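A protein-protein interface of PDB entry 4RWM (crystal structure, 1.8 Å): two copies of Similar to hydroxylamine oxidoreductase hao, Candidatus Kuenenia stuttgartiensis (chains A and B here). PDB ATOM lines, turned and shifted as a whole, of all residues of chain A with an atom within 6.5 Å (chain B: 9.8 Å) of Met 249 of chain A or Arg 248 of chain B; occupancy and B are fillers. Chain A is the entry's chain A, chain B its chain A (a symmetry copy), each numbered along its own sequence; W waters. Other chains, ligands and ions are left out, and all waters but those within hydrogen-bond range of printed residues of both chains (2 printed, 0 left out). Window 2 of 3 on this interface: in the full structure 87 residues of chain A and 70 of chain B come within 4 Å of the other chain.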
ATOM      1  N   LYS A 214       3.760  18.968  12.163  1.00  0.00           N
ATOM      2  CA  LYS A 214       5.038  19.676  12.264  1.00  0.00           C
ATOM      3  C   LYS A 214       5.998  19.222  11.156  1.00  0.00           C
ATOM      4  O   LYS A 214       5.911  18.090  10.688  1.00  0.00           O
ATOM      5  CB  LYS A 214       5.664  19.441  13.644  1.00  0.00           C
ATOM      6  CG  LYS A 214       4.746  19.823  14.808  1.00  0.00           C
ATOM      7  CD  LYS A 214       5.400  19.632  16.171  1.00  0.00           C
ATOM      8  CE  LYS A 214       4.418  20.016  17.286  1.00  0.00           C
ATOM      9  NZ  LYS A 214       4.984  19.990  18.671  1.00  0.00           N
ATOM     10  N   LEU A 241       9.817  31.369  10.444  1.00  0.00           N
ATOM     11  CA  LEU A 241       8.629  31.624  11.268  1.00  0.00           C
ATOM     12  C   LEU A 241       8.149  30.370  12.002  1.00  0.00           C
ATOM     13  O   LEU A 241       7.695  30.461  13.142  1.00  0.00           O
ATOM     14  CB  LEU A 241       7.505  32.232  10.431  1.00  0.00           C
ATOM     15  CG  LEU A 241       7.719  33.671   9.959  1.00  0.00           C
ATOM     16  CD1 LEU A 241       6.497  34.146   9.194  1.00  0.00           C
ATOM     17  CD2 LEU A 241       8.027  34.612  11.122  1.00  0.00           C
ATOM     18  N   TYR A 242       8.262  29.205  11.362  1.00  0.00           N
ATOM     19  CA  TYR A 242       8.013  27.932  12.055  1.00  0.00           C
ATOM     20  C   TYR A 242       8.886  27.824  13.304  1.00  0.00           C
ATOM     21  O   TYR A 242       8.386  27.529  14.397  1.00  0.00           O
ATOM     22  CB  TYR A 242       8.260  26.720  11.139  1.00  0.00           C
ATOM     23  CG  TYR A 242       8.707  25.491  11.901  1.00  0.00           C
ATOM     24  CD1 TYR A 242       7.824  24.804  12.731  1.00  0.00           C
ATOM     25  CD2 TYR A 242      10.022  25.042  11.826  1.00  0.00           C
ATOM     26  CE1 TYR A 242       8.239  23.685  13.456  1.00  0.00           C
ATOM     27  CE2 TYR A 242      10.445  23.931  12.547  1.00  0.00           C
ATOM     28  CZ  TYR A 242       9.549  23.259  13.355  1.00  0.00           C
ATOM     29  OH  TYR A 242       9.976  22.162  14.067  1.00  0.00           O
ATOM     30  N   GLU A 245       7.730  30.374  15.962  1.00  0.00           N
ATOM     31  CA  GLU A 245       6.386  30.228  16.527  1.00  0.00           C
ATOM     32  C   GLU A 245       6.049  28.833  17.056  1.00  0.00           C
ATOM     33  O   GLU A 245       5.035  28.664  17.738  1.00  0.00           O
ATOM     34  CB  GLU A 245       5.333  30.665  15.500  1.00  0.00           C
ATOM     35  CG  GLU A 245       5.485  32.130  15.097  1.00  0.00           C
ATOM     36  CD  GLU A 245       4.233  32.753  14.489  1.00  0.00           C
ATOM     37  OE1 GLU A 245       4.291  33.964  14.200  1.00  0.00           O
ATOM     38  OE2 GLU A 245       3.204  32.063  14.300  1.00  0.00           O
ATOM     39  N   SER A 246       6.889  27.843  16.767  1.00  0.00           N
ATOM     40  CA  SER A 246       6.561  26.456  17.105  1.00  0.00           C
ATOM     41  C   SER A 246       6.219  26.234  18.580  1.00  0.00           C
ATOM     42  O   SER A 246       5.307  25.463  18.899  1.00  0.00           O
ATOM     43  CB  SER A 246       7.700  25.510  16.723  1.00  0.00           C
ATOM     44  OG  SER A 246       7.327  24.172  17.020  1.00  0.00           O
ATOM     45  N   ALA A 247       6.958  26.896  19.468  1.00  0.00           N
ATOM     46  CA  ALA A 247       6.843  26.652  20.906  1.00  0.00           C
ATOM     47  C   ALA A 247       5.510  27.111  21.481  1.00  0.00           C
ATOM     48  O   ALA A 247       5.030  26.535  22.462  1.00  0.00           O
ATOM     49  CB  ALA A 247       7.994  27.328  21.659  1.00  0.00           C
ATOM     50  N   ARG A 248       4.917  28.140  20.882  1.00  0.00           N
ATOM     51  CA  ARG A 248       3.726  28.770  21.457  1.00  0.00           C
ATOM     52  C   ARG A 248       2.463  28.670  20.595  1.00  0.00           C
ATOM     53  O   ARG A 248       1.368  28.980  21.069  1.00  0.00           O
ATOM     54  CB  ARG A 248       4.046  30.223  21.794  1.00  0.00           C
ATOM     55  CG  ARG A 248       5.121  30.341  22.868  1.00  0.00           C
ATOM     56  CD  ARG A 248       5.637  31.758  23.026  1.00  0.00           C
ATOM     57  NE  ARG A 248       6.741  31.819  23.985  1.00  0.00           N
ATOM     58  CZ  ARG A 248       8.013  31.508  23.717  1.00  0.00           C
ATOM     59  NH1 ARG A 248       8.381  31.088  22.506  1.00  0.00           N
ATOM     60  NH2 ARG A 248       8.928  31.616  24.674  1.00  0.00           N
ATOM     61  N   MET A 249       2.604  28.221  19.349  1.00  0.00           N
ATOM     62  CA  MET A 249       1.458  28.098  18.452  1.00  0.00           C
ATOM     63  C   MET A 249       0.623  26.862  18.787  1.00  0.00           C
ATOM     64  O   MET A 249       1.090  25.923  19.442  1.00  0.00           O
ATOM     65  CB  MET A 249       1.907  28.075  16.983  1.00  0.00           C
ATOM     66  CG  MET A 249       2.719  26.859  16.574  1.00  0.00           C
ATOM     67  SD  MET A 249       3.443  27.083  14.937  1.00  0.00           S
ATOM     68  CE  MET A 249       2.114  26.415  13.929  1.00  0.00           C
ATOM     69  N   ASP A 250      -0.622  26.873  18.330  1.00  0.00           N
ATOM     70  CA  ASP A 250      -1.564  25.806  18.626  1.00  0.00           C
ATOM     71  C   ASP A 250      -1.515  24.770  17.512  1.00  0.00           C
ATOM     72  O   ASP A 250      -2.106  24.961  16.452  1.00  0.00           O
ATOM     73  CB  ASP A 250      -2.977  26.383  18.773  1.00  0.00           C
ATOM     74  CG  ASP A 250      -4.003  25.341  19.197  1.00  0.00           C
ATOM     75  OD1 ASP A 250      -5.169  25.729  19.419  1.00  0.00           O
ATOM     76  OD2 ASP A 250      -3.660  24.147  19.315  1.00  0.00           O
ATOM     77  N   TRP A 251      -0.797  23.678  17.766  1.00  0.00           N
ATOM     78  CA  TRP A 251      -0.667  22.580  16.808  1.00  0.00           C
ATOM     79  C   TRP A 251      -1.860  21.619  16.835  1.00  0.00           C
ATOM     80  O   TRP A 251      -1.912  20.672  16.052  1.00  0.00           O
ATOM     81  CB  TRP A 251       0.602  21.782  17.097  1.00  0.00           C
ATOM     82  CG  TRP A 251       1.864  22.517  16.811  1.00  0.00           C
ATOM     83  CD1 TRP A 251       2.682  23.120  17.719  1.00  0.00           C
ATOM     84  CD2 TRP A 251       2.476  22.705  15.527  1.00  0.00           C
ATOM     85  NE1 TRP A 251       3.771  23.675  17.078  1.00  0.00           N
ATOM     86  CE2 TRP A 251       3.664  23.438  15.734  1.00  0.00           C
ATOM     87  CE3 TRP A 251       2.128  22.335  14.220  1.00  0.00           C
ATOM     88  CZ2 TRP A 251       4.510  23.802  14.680  1.00  0.00           C
ATOM     89  CZ3 TRP A 251       2.965  22.702  13.176  1.00  0.00           C
ATOM     90  CH2 TRP A 251       4.143  23.429  13.413  1.00  0.00           C
ATOM     91  N   GLY A 252      -2.793  21.844  17.756  1.00  0.00           N
ATOM     92  CA  GLY A 252      -3.993  21.020  17.856  1.00  0.00           C
ATOM     93  C   GLY A 252      -5.070  21.358  16.844  1.00  0.00           C
ATOM     94  O   GLY A 252      -6.058  20.635  16.739  1.00  0.00           O
ATOM     95  N   TYR A 260      -3.842  28.409  10.707  1.00  0.00           N
ATOM     96  CA  TYR A 260      -2.393  28.578  10.860  1.00  0.00           C
ATOM     97  C   TYR A 260      -1.879  29.871  10.242  1.00  0.00           C
ATOM     98  O   TYR A 260      -2.306  30.262   9.156  1.00  0.00           O
ATOM     99  CB  TYR A 260      -1.657  27.384  10.241  1.00  0.00           C
ATOM    100  CG  TYR A 260      -1.792  26.151  11.098  1.00  0.00           C
ATOM    101  CD1 TYR A 260      -0.860  25.870  12.085  1.00  0.00           C
ATOM    102  CD2 TYR A 260      -2.881  25.295  10.953  1.00  0.00           C
ATOM    103  CE1 TYR A 260      -0.997  24.758  12.902  1.00  0.00           C
ATOM    104  CE2 TYR A 260      -3.030  24.183  11.770  1.00  0.00           C
ATOM    105  CZ  TYR A 260      -2.083  23.922  12.740  1.00  0.00           C
ATOM    106  OH  TYR A 260      -2.216  22.826  13.556  1.00  0.00           O
ATOM    107  N   ARG A 261      -0.955  30.525  10.941  1.00  0.00           N
ATOM    108  CA  ARG A 261      -0.199  31.629  10.358  1.00  0.00           C
ATOM    109  C   ARG A 261       0.943  31.104   9.492  1.00  0.00           C
ATOM    110  O   ARG A 261       1.190  31.620   8.405  1.00  0.00           O
ATOM    111  CB  ARG A 261       0.390  32.542  11.434  1.00  0.00           C
ATOM    112  CG  ARG A 261       1.110  33.727  10.817  1.00  0.00           C
ATOM    113  CD  ARG A 261       1.824  34.606  11.799  1.00  0.00           C
ATOM    114  NE  ARG A 261       2.307  35.809  11.114  1.00  0.00           N
ATOM    115  CZ  ARG A 261       3.469  36.419  11.339  1.00  0.00           C
ATOM    116  NH1 ARG A 261       4.346  35.953  12.233  1.00  0.00           N
ATOM    117  NH2 ARG A 261       3.768  37.506  10.639  1.00  0.00           N
ATOM    118  N   VAL A 262       1.660  30.107  10.006  1.00  0.00           N
ATOM    119  CA  VAL A 262       2.849  29.579   9.349  1.00  0.00           C
ATOM    120  C   VAL A 262       2.502  28.252   8.684  1.00  0.00           C
ATOM    121  O   VAL A 262       2.008  27.342   9.356  1.00  0.00           O
ATOM    122  CB  VAL A 262       3.988  29.342  10.364  1.00  0.00           C
ATOM    123  CG1 VAL A 262       5.212  28.739   9.667  1.00  0.00           C
ATOM    124  CG2 VAL A 262       4.351  30.647  11.083  1.00  0.00           C
ATOM    125  N   THR A 264       3.298  24.612   7.031  1.00  0.00           N
ATOM    126  CA  THR A 264       4.271  23.530   7.129  1.00  0.00           C
ATOM    127  C   THR A 264       4.109  22.600   5.927  1.00  0.00           C
ATOM    128  O   THR A 264       3.184  22.772   5.124  1.00  0.00           O
ATOM    129  CB  THR A 264       4.045  22.697   8.395  1.00  0.00           C
ATOM    130  OG1 THR A 264       2.746  22.082   8.330  1.00  0.00           O
ATOM    131  CG2 THR A 264       4.153  23.565   9.663  1.00  0.00           C
ATOM    132  N   LYS B 214      19.358  18.309  27.726  1.00  0.00           N
ATOM    133  CA  LYS B 214      19.014  18.603  26.334  1.00  0.00           C
ATOM    134  C   LYS B 214      20.210  18.334  25.412  1.00  0.00           C
ATOM    135  O   LYS B 214      21.356  18.437  25.839  1.00  0.00           O
ATOM    136  CB  LYS B 214      18.553  20.059  26.201  1.00  0.00           C
ATOM    137  CG  LYS B 214      17.391  20.424  27.129  1.00  0.00           C
ATOM    138  CD  LYS B 214      16.910  21.858  26.949  1.00  0.00           C
ATOM    139  CE  LYS B 214      15.761  22.156  27.922  1.00  0.00           C
ATOM    140  NZ  LYS B 214      15.118  23.497  27.758  1.00  0.00           N
ATOM    141  N   LEU B 241      11.781  13.897  16.931  1.00  0.00           N
ATOM    142  CA  LEU B 241      10.855  13.937  18.069  1.00  0.00           C
ATOM    143  C   LEU B 241      11.333  14.881  19.175  1.00  0.00           C
ATOM    144  O   LEU B 241      10.515  15.550  19.807  1.00  0.00           O
ATOM    145  CB  LEU B 241      10.604  12.533  18.618  1.00  0.00           C
ATOM    146  CG  LEU B 241       9.775  11.602  17.732  1.00  0.00           C
ATOM    147  CD1 LEU B 241       9.568  10.275  18.438  1.00  0.00           C
ATOM    148  CD2 LEU B 241       8.434  12.225  17.351  1.00  0.00           C
ATOM    149  N   TYR B 242      12.646  14.947  19.399  1.00  0.00           N
ATOM    150  CA  TYR B 242      13.211  15.963  20.300  1.00  0.00           C
ATOM    151  C   TYR B 242      12.776  17.362  19.866  1.00  0.00           C
ATOM    152  O   TYR B 242      12.283  18.149  20.684  1.00  0.00           O
ATOM    153  CB  TYR B 242      14.747  15.889  20.360  1.00  0.00           C
ATOM    154  CG  TYR B 242      15.388  17.230  20.644  1.00  0.00           C
ATOM    155  CD1 TYR B 242      15.273  17.827  21.898  1.00  0.00           C
ATOM    156  CD2 TYR B 242      16.070  17.922  19.648  1.00  0.00           C
ATOM    157  CE1 TYR B 242      15.840  19.076  22.157  1.00  0.00           C
ATOM    158  CE2 TYR B 242      16.636  19.168  19.896  1.00  0.00           C
ATOM    159  CZ  TYR B 242      16.519  19.735  21.150  1.00  0.00           C
ATOM    160  OH  TYR B 242      17.079  20.968  21.387  1.00  0.00           O
ATOM    161  N   GLU B 243      12.950  17.673  18.583  1.00  0.00           N
ATOM    162  CA  GLU B 243      12.573  18.989  18.067  1.00  0.00           C
ATOM    163  C   GLU B 243      11.074  19.237  18.229  1.00  0.00           C
ATOM    164  O   GLU B 243      10.658  20.330  18.624  1.00  0.00           O
ATOM    165  CB  GLU B 243      12.994  19.153  16.598  1.00  0.00           C
ATOM    166  CG  GLU B 243      12.655  20.527  16.009  1.00  0.00           C
ATOM    167  CD  GLU B 243      13.096  20.697  14.562  1.00  0.00           C
ATOM    168  OE1 GLU B 243      14.031  19.999  14.115  1.00  0.00           O
ATOM    169  OE2 GLU B 243      12.505  21.558  13.872  1.00  0.00           O
ATOM    170  N   ALA B 244      10.273  18.211  17.950  1.00  0.00           N
ATOM    171  CA  ALA B 244       8.819  18.303  18.075  1.00  0.00           C
ATOM    172  C   ALA B 244       8.345  18.502  19.521  1.00  0.00           C
ATOM    173  O   ALA B 244       7.400  19.254  19.763  1.00  0.00           O
ATOM    174  CB  ALA B 244       8.161  17.057  17.474  1.00  0.00           C
ATOM    175  N   GLU B 245       8.992  17.830  20.473  1.00  0.00           N
ATOM    176  CA  GLU B 245       8.499  17.781  21.852  1.00  0.00           C
ATOM    177  C   GLU B 245       9.235  18.685  22.841  1.00  0.00           C
ATOM    178  O   GLU B 245       8.764  18.877  23.965  1.00  0.00           O
ATOM    179  CB  GLU B 245       8.507  16.334  22.363  1.00  0.00           C
ATOM    180  CG  GLU B 245       7.604  15.419  21.537  1.00  0.00           C
ATOM    181  CD  GLU B 245       7.184  14.136  22.247  1.00  0.00           C
ATOM    182  OE1 GLU B 245       6.398  13.388  21.635  1.00  0.00           O
ATOM    183  OE2 GLU B 245       7.618  13.868  23.392  1.00  0.00           O
ATOM    184  N   SER B 246      10.366  19.253  22.434  1.00  0.00           N
ATOM    185  CA  SER B 246      11.206  20.008  23.367  1.00  0.00           C
ATOM    186  C   SER B 246      10.472  21.129  24.106  1.00  0.00           C
ATOM    187  O   SER B 246      10.708  21.348  25.300  1.00  0.00           O
ATOM    188  CB  SER B 246      12.421  20.608  22.657  1.00  0.00           C
ATOM    189  OG  SER B 246      13.236  21.289  23.601  1.00  0.00           O
ATOM    190  N   ALA B 247       9.602  21.841  23.393  1.00  0.00           N
ATOM    191  CA  ALA B 247       8.955  23.038  23.931  1.00  0.00           C
ATOM    192  C   ALA B 247       7.977  22.729  25.056  1.00  0.00           C
ATOM    193  O   ALA B 247       7.775  23.562  25.944  1.00  0.00           O
ATOM    194  CB  ALA B 247       8.239  23.809  22.817  1.00  0.00           C
ATOM    195  N   ARG B 248       7.372  21.545  25.020  1.00  0.00           N
ATOM    196  CA  ARG B 248       6.287  21.218  25.950  1.00  0.00           C
ATOM    197  C   ARG B 248       6.584  20.056  26.903  1.00  0.00           C
ATOM    198  O   ARG B 248       5.833  19.834  27.856  1.00  0.00           O
ATOM    199  CB  ARG B 248       5.011  20.964  25.156  1.00  0.00           C
ATOM    200  CG  ARG B 248       4.539  22.207  24.411  1.00  0.00           C
ATOM    201  CD  ARG B 248       3.434  21.909  23.416  1.00  0.00           C
ATOM    202  NE  ARG B 248       3.079  23.100  22.642  1.00  0.00           N
ATOM    203  CZ  ARG B 248       3.753  23.559  21.582  1.00  0.00           C
ATOM    204  NH1 ARG B 248       4.853  22.945  21.144  1.00  0.00           N
ATOM    205  NH2 ARG B 248       3.322  24.647  20.956  1.00  0.00           N
ATOM    206  N   MET B 249       7.678  19.333  26.669  1.00  0.00           N
ATOM    207  CA  MET B 249       8.038  18.202  27.520  1.00  0.00           C
ATOM    208  C   MET B 249       8.650  18.675  28.840  1.00  0.00           C
ATOM    209  O   MET B 249       9.126  19.810  28.963  1.00  0.00           O
ATOM    210  CB  MET B 249       8.986  17.240  26.789  1.00  0.00           C
ATOM    211  CG  MET B 249      10.359  17.803  26.471  1.00  0.00           C
ATOM    212  SD  MET B 249      11.267  16.713  25.356  1.00  0.00           S
ATOM    213  CE  MET B 249      12.082  15.664  26.564  1.00  0.00           C
ATOM    214  N   ASP B 250       8.633  17.789  29.826  1.00  0.00           N
ATOM    215  CA  ASP B 250       9.110  18.110  31.162  1.00  0.00           C
ATOM    216  C   ASP B 250      10.576  17.717  31.279  1.00  0.00           C
ATOM    217  O   ASP B 250      10.898  16.548  31.474  1.00  0.00           O
ATOM    218  CB  ASP B 250       8.263  17.377  32.209  1.00  0.00           C
ATOM    219  CG  ASP B 250       8.630  17.752  33.639  1.00  0.00           C
ATOM    220  OD1 ASP B 250       7.944  17.265  34.562  1.00  0.00           O
ATOM    221  OD2 ASP B 250       9.586  18.526  33.849  1.00  0.00           O
ATOM    222  N   TRP B 251      11.454  18.709  31.148  1.00  0.00           N
ATOM    223  CA  TRP B 251      12.898  18.501  31.256  1.00  0.00           C
ATOM    224  C   TRP B 251      13.390  18.458  32.706  1.00  0.00           C
ATOM    225  O   TRP B 251      14.575  18.244  32.953  1.00  0.00           O
ATOM    226  CB  TRP B 251      13.642  19.619  30.528  1.00  0.00           C
ATOM    227  CG  TRP B 251      13.493  19.589  29.048  1.00  0.00           C
ATOM    228  CD1 TRP B 251      12.674  20.375  28.293  1.00  0.00           C
ATOM    229  CD2 TRP B 251      14.203  18.746  28.130  1.00  0.00           C
ATOM    230  NE1 TRP B 251      12.831  20.074  26.955  1.00  0.00           N
ATOM    231  CE2 TRP B 251      13.759  19.075  26.831  1.00  0.00           C
ATOM    232  CE3 TRP B 251      15.164  17.736  28.281  1.00  0.00           C
ATOM    233  CZ2 TRP B 251      14.250  18.432  25.688  1.00  0.00           C
ATOM    234  CZ3 TRP B 251      15.644  17.096  27.148  1.00  0.00           C
ATOM    235  CH2 TRP B 251      15.186  17.447  25.867  1.00  0.00           C
ATOM    236  N   GLY B 252      12.488  18.694  33.655  1.00  0.00           N
ATOM    237  CA  GLY B 252      12.828  18.643  35.073  1.00  0.00           C
ATOM    238  C   GLY B 252      12.901  17.242  35.649  1.00  0.00           C
ATOM    239  O   GLY B 252      13.322  17.072  36.790  1.00  0.00           O
ATOM    240  N   LYS B 253      12.489  16.238  34.876  1.00  0.00           N
ATOM    241  CA  LYS B 253      12.553  14.852  35.327  1.00  0.00           C
ATOM    242  C   LYS B 253      13.978  14.301  35.225  1.00  0.00           C
ATOM    243  O   LYS B 253      14.708  14.593  34.271  1.00  0.00           O
ATOM    244  CB  LYS B 253      11.578  13.981  34.526  1.00  0.00           C
ATOM    245  CG  LYS B 253      10.112  14.321  34.785  1.00  0.00           C
ATOM    246  CD  LYS B 253       9.176  13.355  34.080  1.00  0.00           C
ATOM    247  CE  LYS B 253       7.732  13.527  34.558  1.00  0.00           C
ATOM    248  NZ  LYS B 253       6.796  12.589  33.857  1.00  0.00           N
ATOM    249  N   TYR B 260      11.042   9.737  30.255  1.00  0.00           N
ATOM    250  CA  TYR B 260      11.133  10.385  28.943  1.00  0.00           C
ATOM    251  C   TYR B 260      10.567   9.530  27.818  1.00  0.00           C
ATOM    252  O   TYR B 260      10.780   8.319  27.781  1.00  0.00           O
ATOM    253  CB  TYR B 260      12.593  10.742  28.634  1.00  0.00           C
ATOM    254  CG  TYR B 260      13.057  11.917  29.455  1.00  0.00           C
ATOM    255  CD1 TYR B 260      12.921  13.212  28.979  1.00  0.00           C
ATOM    256  CD2 TYR B 260      13.585  11.733  30.731  1.00  0.00           C
ATOM    257  CE1 TYR B 260      13.312  14.300  29.744  1.00  0.00           C
ATOM    258  CE2 TYR B 260      13.973  12.817  31.507  1.00  0.00           C
ATOM    259  CZ  TYR B 260      13.834  14.095  31.004  1.00  0.00           C
ATOM    260  OH  TYR B 260      14.214  15.177  31.760  1.00  0.00           O
HETATM  261  O   HOH W   1       8.981  22.159  16.698  1.00  0.00           O
HETATM  262  O   HOH W   2       6.596  22.399  19.046  1.00  0.00           O
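NZ of Lys 214 of chain A sits at hydrogen-bond distance from O of Ala 244 of chain B. OE2 of Glu 243 of chain B sits at hydrogen-bond distance from OH of Tyr 242 of chain A (2.6 Å). O of Ser 246 of chain A is in hydrogen-bond range of NH2 of Arg 248 of chain B (3.0 Å). O of Ala 247 of chain A sits at hydrogen-bond distance from NH2 of Arg 248 of chain B, at 3.0 Å. The backbone carbonyl oxygen of Met 249 of chain A is in hydrogen-bond range of the guanidinium group of Arg 248 of chain B.
Of chain B, only Arg 248 (3.0 Å) comes within 4 Å of Met 249 of chain A. Printed residues of chain A within 4 Å of Arg 248 of chain B: Lys 214, Ser 246, Ala 247, Arg 248, Met 249 and Trp 251. Ser 246 of chain A touches just one residue of chain B: Arg 248. Of the printed residues of chain B, Ala 247 of chain A touches Ala 247 and Arg 248. Printed residues of chain B within 4 Å of Trp 251 of chain A: Arg 248 (3.6 Å). Printed residues of chain A within 4 Å of Ala 244 of chain B: Lys 214. The nearest residue of chain A that does not touch Arg 248 of chain B is Asp 250 of chain A (5.2 Å). The nearest printed residue of chain A that does not touch Ala 247 of chain B is Ser 246 of chain A (5.2 Å).
Lys 214 of chain A touches Arg 248 of chain B, but with the chains exchanged Arg 248 of chain A does not touch Lys 214 of chain B (10.7 Å). Ser 246 of chain A touches Arg 248 of chain B, but with the chains exchanged Arg 248 of chain A does not touch Ser 246 of chain B (9.5 Å). Arg 248 of chain B touches its own counterpart, Arg 248 of chain A. Met 249 of chain A touches Arg 248 of chain B, but with the chains exchanged Arg 248 of chain A does not touch Met 249 of chain B (10.9 Å). 12 positions are printed for both chains. Of the 9 pairs that touch across the chains among the printed residues, 2 have their exchanged pair printed and touching as well.
Hydrophobic or aromatic side chains of chain B within 4 Å of the printed part of chain A: Ala 244 and Ala 247. Along chain B the printed residues that touch a printed residue of chain A span positions 243 to 248. Printed residues of chain A that touch a printed residue of chain B: Lys 214, Tyr 242, Ser 246, Ala 247, Arg 248, Met 249 and Trp 251. Hydrophobic or aromatic side chains of chain A within 4 Å of the printed part of chain B: Tyr 242, Ala 247 and Trp 251.
Water W1 lies within hydrogen-bond range of OG of Ser 246 of chain A (2.6 Å), OH of Tyr 242 of chain A (2.8 Å) and O of Glu 243 of chain B (3.1 Å). Water W2 lies within hydrogen-bond range of the guanidinium group (NH1) of Arg 248 of chain B (2.8 Å), the side-chain hydroxyl (OG) of Ser 246 of chain A (2.8 Å), the side-chain amino group (NZ) of Lys 214 of chain A (2.9 Å) and the backbone carbonyl oxygen (O) of Ala 244 of chain B (3.3 Å).
NZ of Lys 214 of chain A touches NH1 of Arg 248 of chain B (3.9 Å). Ala 247 of chain A touches Ala 247 of chain B (CA to CB, 3.7 Å). NH2 of Arg 248 of chain B touches N of Arg 248 of chain A, 3.8 Å away. Trp 251 of chain A touches Arg 248 of chain B.
The backbone carbonyl oxygen (O) of Ser 246 of chain A lies within hydrogen-bond range of the indole nitrogen (NE1) of Trp 251 of chain A, 3.0 Å away. O of Trp 251 of chain A lies within hydrogen-bond range of OH of Tyr 260 of chain A (3.3 Å).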
